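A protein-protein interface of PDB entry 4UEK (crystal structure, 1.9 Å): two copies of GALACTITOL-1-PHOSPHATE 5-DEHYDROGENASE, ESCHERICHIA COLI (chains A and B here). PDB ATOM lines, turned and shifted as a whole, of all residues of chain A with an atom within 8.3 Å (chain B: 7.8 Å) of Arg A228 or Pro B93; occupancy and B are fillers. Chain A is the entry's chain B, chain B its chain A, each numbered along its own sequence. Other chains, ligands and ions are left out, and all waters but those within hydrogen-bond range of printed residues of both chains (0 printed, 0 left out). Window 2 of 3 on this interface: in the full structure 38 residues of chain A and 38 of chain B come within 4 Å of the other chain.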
ATOM      1  N   ASN A 163      17.377  -0.646   9.151  1.00  0.00           N
ATOM      2  CA  ASN A 163      16.473  -0.153   8.132  1.00  0.00           C
ATOM      3  C   ASN A 163      16.574  -1.065   6.902  1.00  0.00           C
ATOM      4  O   ASN A 163      17.520  -0.977   6.119  1.00  0.00           O
ATOM      5  CB  ASN A 163      16.806   1.301   7.793  1.00  0.00           C
ATOM      6  CG  ASN A 163      16.513   2.250   8.936  1.00  0.00           C
ATOM      7  OD1 ASN A 163      15.416   2.237   9.503  1.00  0.00           O
ATOM      8  ND2 ASN A 163      17.493   3.087   9.285  1.00  0.00           N
ATOM      9  N   ILE A 165      15.629  -2.787   3.270  1.00  0.00           N
ATOM     10  CA  ILE A 165      15.118  -2.431   1.956  1.00  0.00           C
ATOM     11  C   ILE A 165      15.097  -3.701   1.127  1.00  0.00           C
ATOM     12  O   ILE A 165      16.147  -4.310   0.881  1.00  0.00           O
ATOM     13  CB  ILE A 165      15.987  -1.349   1.273  1.00  0.00           C
ATOM     14  CG1 ILE A 165      16.098  -0.120   2.189  1.00  0.00           C
ATOM     15  CG2 ILE A 165      15.397  -0.970  -0.095  1.00  0.00           C
ATOM     16  CD1 ILE A 165      16.869   1.048   1.594  1.00  0.00           C
ATOM     17  N   SER A 187      12.709  -0.490  10.375  1.00  0.00           N
ATOM     18  CA  SER A 187      11.791  -0.135   9.306  1.00  0.00           C
ATOM     19  C   SER A 187      11.960  -1.108   8.131  1.00  0.00           C
ATOM     20  O   SER A 187      13.000  -1.758   7.992  1.00  0.00           O
ATOM     21  CB  SER A 187      12.029   1.312   8.856  1.00  0.00           C
ATOM     22  OG  SER A 187      13.284   1.434   8.189  1.00  0.00           O
ATOM     23  N   GLN A 221      16.607   8.219  -2.874  1.00  0.00           N
ATOM     24  CA  GLN A 221      17.603   8.521  -1.855  1.00  0.00           C
ATOM     25  C   GLN A 221      17.147   9.707  -1.019  1.00  0.00           C
ATOM     26  O   GLN A 221      17.302   9.720   0.201  1.00  0.00           O
ATOM     27  CB  GLN A 221      18.973   8.792  -2.498  1.00  0.00           C
ATOM     28  CG  GLN A 221      20.110   8.766  -1.501  1.00  0.00           C
ATOM     29  CD  GLN A 221      21.477   8.712  -2.153  1.00  0.00           C
ATOM     30  OE1 GLN A 221      21.622   8.955  -3.348  1.00  0.00           O
ATOM     31  NE2 GLN A 221      22.487   8.388  -1.365  1.00  0.00           N
ATOM     32  N   SER A 222      16.551  10.698  -1.673  1.00  0.00           N
ATOM     33  CA  SER A 222      16.030  11.834  -0.944  1.00  0.00           C
ATOM     34  C   SER A 222      14.977  11.411   0.087  1.00  0.00           C
ATOM     35  O   SER A 222      14.999  11.881   1.217  1.00  0.00           O
ATOM     36  CB  SER A 222      15.449  12.870  -1.906  1.00  0.00           C
ATOM     37  OG  SER A 222      14.796  13.889  -1.178  1.00  0.00           O
ATOM     38  N   VAL A 223      14.067  10.522  -0.289  1.00  0.00           N
ATOM     39  CA  VAL A 223      13.068  10.054   0.673  1.00  0.00           C
ATOM     40  C   VAL A 223      13.733   9.248   1.810  1.00  0.00           C
ATOM     41  O   VAL A 223      13.294   9.305   2.959  1.00  0.00           O
ATOM     42  CB  VAL A 223      11.972   9.195  -0.010  1.00  0.00           C
ATOM     43  CG1 VAL A 223      11.012   8.641   1.025  1.00  0.00           C
ATOM     44  CG2 VAL A 223      11.189  10.021  -1.032  1.00  0.00           C
ATOM     45  N   LEU A 224      14.804   8.524   1.489  1.00  0.00           N
ATOM     46  CA  LEU A 224      15.467   7.639   2.458  1.00  0.00           C
ATOM     47  C   LEU A 224      16.420   8.324   3.420  1.00  0.00           C
ATOM     48  O   LEU A 224      16.993   7.661   4.284  1.00  0.00           O
ATOM     49  CB  LEU A 224      16.253   6.551   1.738  1.00  0.00           C
ATOM     50  CG  LEU A 224      15.424   5.470   1.046  1.00  0.00           C
ATOM     51  CD1 LEU A 224      16.339   4.597   0.210  1.00  0.00           C
ATOM     52  CD2 LEU A 224      14.666   4.654   2.079  1.00  0.00           C
ATOM     53  N   ARG A 225      16.599   9.632   3.264  1.00  0.00           N
ATOM     54  CA  ARG A 225      17.559  10.388   4.067  1.00  0.00           C
ATOM     55  C   ARG A 225      17.484  10.110   5.564  1.00  0.00           C
ATOM     56  O   ARG A 225      18.502   9.868   6.202  1.00  0.00           O
ATOM     57  CB  ARG A 225      17.375  11.893   3.835  1.00  0.00           C
ATOM     58  CG  ARG A 225      17.970  12.380   2.526  1.00  0.00           C
ATOM     59  CD  ARG A 225      19.484  12.264   2.551  1.00  0.00           C
ATOM     60  NE  ARG A 225      20.112  13.366   3.279  1.00  0.00           N
ATOM     61  CZ  ARG A 225      21.411  13.425   3.562  1.00  0.00           C
ATOM     62  NH1 ARG A 225      22.213  12.438   3.182  1.00  0.00           N
ATOM     63  NH2 ARG A 225      21.904  14.466   4.222  1.00  0.00           N
ATOM     64  N   GLU A 226      16.283  10.154   6.123  1.00  0.00           N
ATOM     65  CA  GLU A 226      16.134   9.980   7.558  1.00  0.00           C
ATOM     66  C   GLU A 226      16.434   8.541   7.959  1.00  0.00           C
ATOM     67  O   GLU A 226      16.709   8.248   9.122  1.00  0.00           O
ATOM     68  CB  GLU A 226      14.721  10.377   8.007  1.00  0.00           C
ATOM     69  CG  GLU A 226      13.620   9.511   7.404  1.00  0.00           C
ATOM     70  CD  GLU A 226      12.216   9.997   7.752  1.00  0.00           C
ATOM     71  OE1 GLU A 226      12.061  10.801   8.704  1.00  0.00           O
ATOM     72  OE2 GLU A 226      11.265   9.561   7.070  1.00  0.00           O
ATOM     73  N   LEU A 227      16.387   7.641   6.986  1.00  0.00           N
ATOM     74  CA  LEU A 227      16.620   6.237   7.261  1.00  0.00           C
ATOM     75  C   LEU A 227      17.885   5.727   6.589  1.00  0.00           C
ATOM     76  O   LEU A 227      17.964   4.536   6.281  1.00  0.00           O
ATOM     77  CB  LEU A 227      15.433   5.398   6.793  1.00  0.00           C
ATOM     78  CG  LEU A 227      14.112   5.636   7.523  1.00  0.00           C
ATOM     79  CD1 LEU A 227      13.081   4.670   6.986  1.00  0.00           C
ATOM     80  CD2 LEU A 227      14.278   5.471   9.028  1.00  0.00           C
ATOM     81  N   ARG A 228      18.869   6.601   6.347  1.00  0.00           N
ATOM     82  CA  ARG A 228      20.011   6.183   5.526  1.00  0.00           C
ATOM     83  C   ARG A 228      21.034   5.359   6.308  1.00  0.00           C
ATOM     84  O   ARG A 228      21.832   4.638   5.715  1.00  0.00           O
ATOM     85  CB  ARG A 228      20.700   7.383   4.866  1.00  0.00           C
ATOM     86  CG  ARG A 228      21.279   8.431   5.805  1.00  0.00           C
ATOM     87  CD  ARG A 228      21.782   9.612   4.990  1.00  0.00           C
ATOM     88  NE  ARG A 228      21.602  10.881   5.699  1.00  0.00           N
ATOM     89  CZ  ARG A 228      22.459  11.310   6.607  1.00  0.00           C
ATOM     90  NH1 ARG A 228      23.497  10.554   6.863  1.00  0.00           N
ATOM     91  NH2 ARG A 228      22.301  12.459   7.244  1.00  0.00           N
ATOM     92  N   PHE A 229      20.985   5.430   7.633  1.00  0.00           N
ATOM     93  CA  PHE A 229      21.904   4.656   8.455  1.00  0.00           C
ATOM     94  C   PHE A 229      21.435   3.241   8.798  1.00  0.00           C
ATOM     95  O   PHE A 229      20.229   2.974   8.928  1.00  0.00           O
ATOM     96  CB  PHE A 229      22.174   5.402   9.743  1.00  0.00           C
ATOM     97  CG  PHE A 229      22.902   6.686   9.541  1.00  0.00           C
ATOM     98  CD1 PHE A 229      24.238   6.679   9.177  1.00  0.00           C
ATOM     99  CD2 PHE A 229      22.259   7.904   9.716  1.00  0.00           C
ATOM    100  CE1 PHE A 229      24.932   7.871   8.995  1.00  0.00           C
ATOM    101  CE2 PHE A 229      22.940   9.094   9.535  1.00  0.00           C
ATOM    102  CZ  PHE A 229      24.285   9.074   9.187  1.00  0.00           C
ATOM    103  N   ASN A 230      22.406   2.352   8.970  1.00  0.00           N
ATOM    104  CA  ASN A 230      22.145   0.974   9.392  1.00  0.00           C
ATOM    105  C   ASN A 230      21.195   0.240   8.445  1.00  0.00           C
ATOM    106  O   ASN A 230      20.269  -0.458   8.867  1.00  0.00           O
ATOM    107  CB  ASN A 230      21.604   0.966  10.820  1.00  0.00           C
ATOM    108  CG  ASN A 230      22.596   1.548  11.816  1.00  0.00           C
ATOM    109  OD1 ASN A 230      23.746   1.119  11.881  1.00  0.00           O
ATOM    110  ND2 ASN A 230      22.152   2.529  12.595  1.00  0.00           N
ATOM    111  N   GLN A 231      21.444   0.409   7.154  1.00  0.00           N
ATOM    112  CA  GLN A 231      20.617  -0.200   6.129  1.00  0.00           C
ATOM    113  C   GLN A 231      21.014  -1.638   5.829  1.00  0.00           C
ATOM    114  O   GLN A 231      22.178  -1.994   5.889  1.00  0.00           O
ATOM    115  CB  GLN A 231      20.688   0.618   4.841  1.00  0.00           C
ATOM    116  CG  GLN A 231      19.822   1.861   4.865  1.00  0.00           C
ATOM    117  CD  GLN A 231      19.855   2.610   3.558  1.00  0.00           C
ATOM    118  OE1 GLN A 231      20.607   2.261   2.639  1.00  0.00           O
ATOM    119  NE2 GLN A 231      19.010   3.627   3.451  1.00  0.00           N
ATOM    120  N   LEU A 232      20.023  -2.449   5.503  1.00  0.00           N
ATOM    121  CA  LEU A 232      20.252  -3.774   4.954  1.00  0.00           C
ATOM    122  C   LEU A 232      19.358  -3.923   3.748  1.00  0.00           C
ATOM    123  O   LEU A 232      18.133  -3.934   3.868  1.00  0.00           O
ATOM    124  CB  LEU A 232      19.964  -4.860   5.979  1.00  0.00           C
ATOM    125  CG  LEU A 232      19.900  -6.279   5.416  1.00  0.00           C
ATOM    126  CD1 LEU A 232      21.226  -6.613   4.720  1.00  0.00           C
ATOM    127  CD2 LEU A 232      19.614  -7.227   6.563  1.00  0.00           C
ATOM    128  N   ILE A 233      19.988  -4.022   2.590  1.00  0.00           N
ATOM    129  CA  ILE A 233      19.287  -4.095   1.320  1.00  0.00           C
ATOM    130  C   ILE A 233      19.385  -5.498   0.733  1.00  0.00           C
ATOM    131  O   ILE A 233      20.481  -6.054   0.585  1.00  0.00           O
ATOM    132  CB  ILE A 233      19.872  -3.073   0.344  1.00  0.00           C
ATOM    133  CG1 ILE A 233      19.903  -1.687   1.008  1.00  0.00           C
ATOM    134  CG2 ILE A 233      19.103  -3.079  -0.985  1.00  0.00           C
ATOM    135  CD1 ILE A 233      20.655  -0.654   0.215  1.00  0.00           C
ATOM    136  N   ILE A 249      21.096   3.938  -4.330  1.00  0.00           N
ATOM    137  CA  ILE A 249      20.231   4.449  -3.266  1.00  0.00           C
ATOM    138  C   ILE A 249      20.831   4.221  -1.893  1.00  0.00           C
ATOM    139  O   ILE A 249      20.368   4.805  -0.922  1.00  0.00           O
ATOM    140  CB  ILE A 249      18.813   3.808  -3.303  1.00  0.00           C
ATOM    141  CG1 ILE A 249      18.864   2.337  -2.886  1.00  0.00           C
ATOM    142  CG2 ILE A 249      18.183   3.975  -4.680  1.00  0.00           C
ATOM    143  CD1 ILE A 249      17.513   1.614  -2.997  1.00  0.00           C
ATOM    144  N   ALA A 250      21.868   3.388  -1.810  1.00  0.00           N
ATOM    145  CA  ALA A 250      22.384   2.951  -0.508  1.00  0.00           C
ATOM    146  C   ALA A 250      22.924   4.116   0.329  1.00  0.00           C
ATOM    147  O   ALA A 250      23.524   5.064  -0.205  1.00  0.00           O
ATOM    148  CB  ALA A 250      23.474   1.899  -0.684  1.00  0.00           C
ATOM    149  N   GLY A 251      22.713   4.036   1.636  1.00  0.00           N
ATOM    150  CA  GLY A 251      23.236   5.042   2.545  1.00  0.00           C
ATOM    151  C   GLY A 251      24.617   4.626   3.022  1.00  0.00           C
ATOM    152  O   GLY A 251      25.137   3.591   2.591  1.00  0.00           O
ATOM    153  N   PRO A 252      25.215   5.417   3.922  1.00  0.00           N
ATOM    154  CA  PRO A 252      26.572   5.135   4.397  1.00  0.00           C
ATOM    155  C   PRO A 252      26.683   3.809   5.140  1.00  0.00           C
ATOM    156  O   PRO A 252      25.853   3.472   6.003  1.00  0.00           O
ATOM    157  CB  PRO A 252      26.875   6.320   5.330  1.00  0.00           C
ATOM    158  CG  PRO A 252      25.571   6.894   5.674  1.00  0.00           C
ATOM    159  CD  PRO A 252      24.676   6.659   4.495  1.00  0.00           C
ATOM    160  N   HIS A 253      27.709   3.051   4.763  1.00  0.00           N
ATOM    161  CA  HIS A 253      28.013   1.745   5.348  1.00  0.00           C
ATOM    162  C   HIS A 253      26.864   0.738   5.308  1.00  0.00           C
ATOM    163  O   HIS A 253      26.800  -0.152   6.150  1.00  0.00           O
ATOM    164  CB  HIS A 253      28.487   1.918   6.792  1.00  0.00           C
ATOM    165  CG  HIS A 253      29.836   2.561   6.899  1.00  0.00           C
ATOM    166  ND1 HIS A 253      30.951   1.876   7.327  1.00  0.00           N
ATOM    167  CD2 HIS A 253      30.251   3.813   6.606  1.00  0.00           C
ATOM    168  CE1 HIS A 253      31.999   2.686   7.305  1.00  0.00           C
ATOM    169  NE2 HIS A 253      31.603   3.867   6.870  1.00  0.00           N
ATOM    170  N   ALA A 254      25.999   0.854   4.302  1.00  0.00           N
ATOM    171  CA  ALA A 254      24.869  -0.055   4.151  1.00  0.00           C
ATOM    172  C   ALA A 254      25.385  -1.448   3.828  1.00  0.00           C
ATOM    173  O   ALA A 254      26.439  -1.599   3.197  1.00  0.00           O
ATOM    174  CB  ALA A 254      23.925   0.432   3.057  1.00  0.00           C
ATOM    175  N   GLN A 255      24.660  -2.458   4.294  1.00  0.00           N
ATOM    176  CA  GLN A 255      24.887  -3.835   3.881  1.00  0.00           C
ATOM    177  C   GLN A 255      23.998  -4.129   2.688  1.00  0.00           C
ATOM    178  O   GLN A 255      22.805  -3.842   2.716  1.00  0.00           O
ATOM    179  CB  GLN A 255      24.573  -4.816   4.998  1.00  0.00           C
ATOM    180  CG  GLN A 255      25.506  -4.809   6.174  1.00  0.00           C
ATOM    181  CD  GLN A 255      24.918  -5.583   7.322  1.00  0.00           C
ATOM    182  OE1 GLN A 255      23.898  -5.182   7.888  1.00  0.00           O
ATOM    183  NE2 GLN A 255      25.535  -6.710   7.664  1.00  0.00           N
ATOM    184  N   LEU A 281      30.317   0.453   1.338  1.00  0.00           N
ATOM    185  CA  LEU A 281      29.292  -0.585   1.398  1.00  0.00           C
ATOM    186  C   LEU A 281      29.902  -1.952   1.697  1.00  0.00           C
ATOM    187  O   LEU A 281      31.096  -2.195   1.468  1.00  0.00           O
ATOM    188  CB  LEU A 281      28.509  -0.646   0.076  1.00  0.00           C
ATOM    189  CG  LEU A 281      27.821   0.650  -0.363  1.00  0.00           C
ATOM    190  CD1 LEU A 281      27.078   0.471  -1.676  1.00  0.00           C
ATOM    191  CD2 LEU A 281      26.863   1.162   0.731  1.00  0.00           C
ATOM    192  N   CYS B  89      33.825  17.793   8.450  1.00  0.00           N
ATOM    193  CA  CYS B  89      33.206  18.933   9.139  1.00  0.00           C
ATOM    194  C   CYS B  89      33.027  18.707  10.644  1.00  0.00           C
ATOM    195  O   CYS B  89      32.876  19.661  11.392  1.00  0.00           O
ATOM    196  CB  CYS B  89      31.854  19.276   8.496  1.00  0.00           C
ATOM    197  SG  CYS B  89      30.461  18.246   9.021  1.00  0.00           S
ATOM    198  N   PHE B  90      33.022  17.445  11.061  1.00  0.00           N
ATOM    199  CA  PHE B  90      32.858  17.016  12.463  1.00  0.00           C
ATOM    200  C   PHE B  90      31.504  17.345  13.109  1.00  0.00           C
ATOM    201  O   PHE B  90      31.340  17.155  14.311  1.00  0.00           O
ATOM    202  CB  PHE B  90      33.991  17.581  13.343  1.00  0.00           C
ATOM    203  CG  PHE B  90      35.363  17.104  12.934  1.00  0.00           C
ATOM    204  CD1 PHE B  90      35.725  15.767  13.098  1.00  0.00           C
ATOM    205  CD2 PHE B  90      36.278  17.978  12.356  1.00  0.00           C
ATOM    206  CE1 PHE B  90      36.972  15.312  12.693  1.00  0.00           C
ATOM    207  CE2 PHE B  90      37.542  17.528  11.952  1.00  0.00           C
ATOM    208  CZ  PHE B  90      37.891  16.210  12.131  1.00  0.00           C
ATOM    209  N   THR B  91      30.522  17.796  12.332  1.00  0.00           N
ATOM    210  CA  THR B  91      29.233  18.173  12.917  1.00  0.00           C
ATOM    211  C   THR B  91      27.998  17.580  12.233  1.00  0.00           C
ATOM    212  O   THR B  91      26.877  17.735  12.740  1.00  0.00           O
ATOM    213  CB  THR B  91      29.052  19.694  12.919  1.00  0.00           C
ATOM    214  OG1 THR B  91      29.026  20.164  11.567  1.00  0.00           O
ATOM    215  CG2 THR B  91      30.190  20.368  13.670  1.00  0.00           C
ATOM    216  N   CYS B  92      28.186  16.910  11.095  1.00  0.00           N
ATOM    217  CA  CYS B  92      27.081  16.171  10.453  1.00  0.00           C
ATOM    218  C   CYS B  92      26.840  14.795  11.113  1.00  0.00           C
ATOM    219  O   CYS B  92      27.665  14.325  11.896  1.00  0.00           O
ATOM    220  CB  CYS B  92      27.360  16.000   8.956  1.00  0.00           C
ATOM    221  SG  CYS B  92      28.717  14.876   8.570  1.00  0.00           S
ATOM    222  N   PRO B  93      25.703  14.146  10.806  1.00  0.00           N
ATOM    223  CA  PRO B  93      25.441  12.848  11.447  1.00  0.00           C
ATOM    224  C   PRO B  93      26.493  11.784  11.100  1.00  0.00           C
ATOM    225  O   PRO B  93      26.823  10.967  11.955  1.00  0.00           O
ATOM    226  CB  PRO B  93      24.067  12.464  10.899  1.00  0.00           C
ATOM    227  CG  PRO B  93      23.400  13.788  10.627  1.00  0.00           C
ATOM    228  CD  PRO B  93      24.511  14.656  10.101  1.00  0.00           C
ATOM    229  N   GLU B  94      27.015  11.812   9.873  1.00  0.00           N
ATOM    230  CA  GLU B  94      28.082  10.893   9.462  1.00  0.00           C
ATOM    231  C   GLU B  94      29.333  11.050  10.338  1.00  0.00           C
ATOM    232  O   GLU B  94      29.875  10.060  10.843  1.00  0.00           O
ATOM    233  CB  GLU B  94      28.435  11.117   7.986  1.00  0.00           C
ATOM    234  CG  GLU B  94      27.491  10.428   6.980  1.00  0.00           C
ATOM    235  CD  GLU B  94      26.196  11.192   6.704  1.00  0.00           C
ATOM    236  OE1 GLU B  94      25.895  12.203   7.374  1.00  0.00           O
ATOM    237  OE2 GLU B  94      25.436  10.762   5.807  1.00  0.00           O
ATOM    238  N   CYS B  95      29.776  12.292  10.530  1.00  0.00           N
ATOM    239  CA  CYS B  95      30.956  12.593  11.358  1.00  0.00           C
ATOM    240  C   CYS B  95      30.742  12.211  12.831  1.00  0.00           C
ATOM    241  O   CYS B  95      31.636  11.659  13.480  1.00  0.00           O
ATOM    242  CB  CYS B  95      31.312  14.083  11.255  1.00  0.00           C
ATOM    243  SG  CYS B  95      32.232  14.593   9.759  1.00  0.00           S
ATOM    244  N   LEU B  96      29.550  12.514  13.347  1.00  0.00           N
ATOM    245  CA  LEU B  96      29.181  12.154  14.711  1.00  0.00           C
ATOM    246  C   LEU B  96      29.169  10.634  14.902  1.00  0.00           C
ATOM    247  O   LEU B  96      29.262  10.141  16.021  1.00  0.00           O
ATOM    248  CB  LEU B  96      27.812  12.758  15.077  1.00  0.00           C
ATOM    249  CG  LEU B  96      27.790  14.295  15.041  1.00  0.00           C
ATOM    250  CD1 LEU B  96      26.471  14.865  15.549  1.00  0.00           C
ATOM    251  CD2 LEU B  96      28.967  14.880  15.824  1.00  0.00           C
ATOM    252  N   LYS B  97      29.086   9.888  13.808  1.00  0.00           N
ATOM    253  CA  LYS B  97      29.157   8.432  13.905  1.00  0.00           C
ATOM    254  C   LYS B  97      30.583   7.918  13.690  1.00  0.00           C
ATOM    255  O   LYS B  97      30.854   6.731  13.837  1.00  0.00           O
ATOM    256  CB  LYS B  97      28.200   7.786  12.902  1.00  0.00           C
ATOM    257  CG  LYS B  97      26.731   7.957  13.297  1.00  0.00           C
ATOM    258  CD  LYS B  97      25.806   7.166  12.393  1.00  0.00           C
ATOM    259  CE  LYS B  97      24.354   7.646  12.514  1.00  0.00           C
ATOM    260  NZ  LYS B  97      23.720   7.395  13.837  1.00  0.00           N
ATOM    261  N   GLY B  98      31.500   8.814  13.357  1.00  0.00           N
ATOM    262  CA  GLY B  98      32.862   8.395  13.095  1.00  0.00           C
ATOM    263  C   GLY B  98      33.030   7.954  11.654  1.00  0.00           C
ATOM    264  O   GLY B  98      34.012   7.307  11.309  1.00  0.00           O
ATOM    265  N   PHE B  99      32.068   8.325  10.815  1.00  0.00           N
ATOM    266  CA  PHE B  99      32.102   8.021   9.395  1.00  0.00           C
ATOM    267  C   PHE B  99      32.748   9.174   8.613  1.00  0.00           C
ATOM    268  O   PHE B  99      32.146   9.707   7.677  1.00  0.00           O
ATOM    269  CB  PHE B  99      30.683   7.769   8.860  1.00  0.00           C
ATOM    270  CG  PHE B  99      29.992   6.557   9.446  1.00  0.00           C
ATOM    271  CD1 PHE B  99      30.695   5.578  10.125  1.00  0.00           C
ATOM    272  CD2 PHE B  99      28.625   6.390   9.277  1.00  0.00           C
ATOM    273  CE1 PHE B  99      30.044   4.461  10.644  1.00  0.00           C
ATOM    274  CE2 PHE B  99      27.976   5.284   9.796  1.00  0.00           C
ATOM    275  CZ  PHE B  99      28.690   4.321  10.484  1.00  0.00           C
ATOM    276  N   GLN B 102      32.650   9.681   4.820  1.00  0.00           N
ATOM    277  CA  GLN B 102      31.340   9.901   4.213  1.00  0.00           C
ATOM    278  C   GLN B 102      30.780  11.298   4.549  1.00  0.00           C
ATOM    279  O   GLN B 102      29.613  11.582   4.253  1.00  0.00           O
ATOM    280  CB  GLN B 102      30.353   8.810   4.659  1.00  0.00           C
ATOM    281  CG  GLN B 102      30.620   7.423   4.064  1.00  0.00           C
ATOM    282  CD  GLN B 102      31.847   6.727   4.641  1.00  0.00           C
ATOM    283  OE1 GLN B 102      32.092   6.760   5.850  1.00  0.00           O
ATOM    284  NE2 GLN B 102      32.625   6.082   3.771  1.00  0.00           N
ATOM    285  N   CYS B 103      31.608  12.157   5.157  1.00  0.00           N
ATOM    286  CA  CYS B 103      31.172  13.513   5.534  1.00  0.00           C
ATOM    287  C   CYS B 103      30.660  14.253   4.314  1.00  0.00           C
ATOM    288  O   CYS B 103      31.310  14.264   3.255  1.00  0.00           O
ATOM    289  CB  CYS B 103      32.298  14.349   6.179  1.00  0.00           C
ATOM    290  SG  CYS B 103      31.868  16.133   6.299  1.00  0.00           S
ATOM    291  N   ALA B 104      29.508  14.885   4.479  1.00  0.00           N
ATOM    292  CA  ALA B 104      28.882  15.636   3.404  1.00  0.00           C
ATOM    293  C   ALA B 104      29.718  16.845   2.981  1.00  0.00           C
ATOM    294  O   ALA B 104      29.662  17.272   1.827  1.00  0.00           O
ATOM    295  CB  ALA B 104      27.486  16.078   3.831  1.00  0.00           C
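OE1 of Glu B94 lies within salt-bridge range of NH1 of Arg A228 (3.0 Å). The side-chain amide oxygen (OE1) of Gln B102 is in hydrogen-bond range of a ring nitrogen (NE2) of His A253.
The side-chain amide nitrogen (ND2) of Asn A163 sits at hydrogen-bond distance from the backbone carbonyl oxygen (O) of Phe A229 (2.8 Å). The guanidinium group of Arg A228 sits close to the backbone carbonyl oxygen of Arg A225, 3.3 Å away. N of Phe B99 is in hydrogen-bond range of O of Glu B94, 2.8 Å away. The backbone carbonyl oxygen of Phe B99 sits close to the side-chain amide oxygen of Gln B102. The backbone NH (N) of Glu B94 lies close to the side-chain sulfur (SG) of Cys B92 (3.7 Å).
Pro B93 touches Arg A228. Pro B93 touches Phe A229 (CB to CZ, 3.8 Å). Glu B94 touches Phe A229 (CD to CZ, 3.8 Å). Phe A229 touches Lys B97. Phe A229 touches Phe B99 (CE1 to CD2, 3.99 Å). Pro A252 touches Glu B94. Phe B99 touches His A253.
Printed residues of chain A within 4 Å of Pro B93: Arg A228 (3.8 Å) and Phe A229 (3.8 Å). No residue of chain A comes within 4 Å of Cys B92. Printed residues of chain A within 4 Å of Lys B97: Phe A229 (3.4 Å). Of the printed residues of chain B, His A253 touches Phe B99 (3.8 Å) and Gln B102 (3.1 Å). Ala A250 touches none of the printed residues of chain B. The nearest printed residue of chain B that does not touch Phe A229 is Cys B95 (6.5 Å).
Hydrophobic or aromatic side chains of chain B within 4 Å of the printed part of chain A: Pro B93 and Phe B99. Among the printed residues, 9 pairs touch across the chains. Among the printed residues, Asp or Glu carboxylates within 4 Å of a Lys or Arg side-chain nitrogen of the other chain: Arg A228 with Glu B94 (2.2 Å).
No position is printed for both chains.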
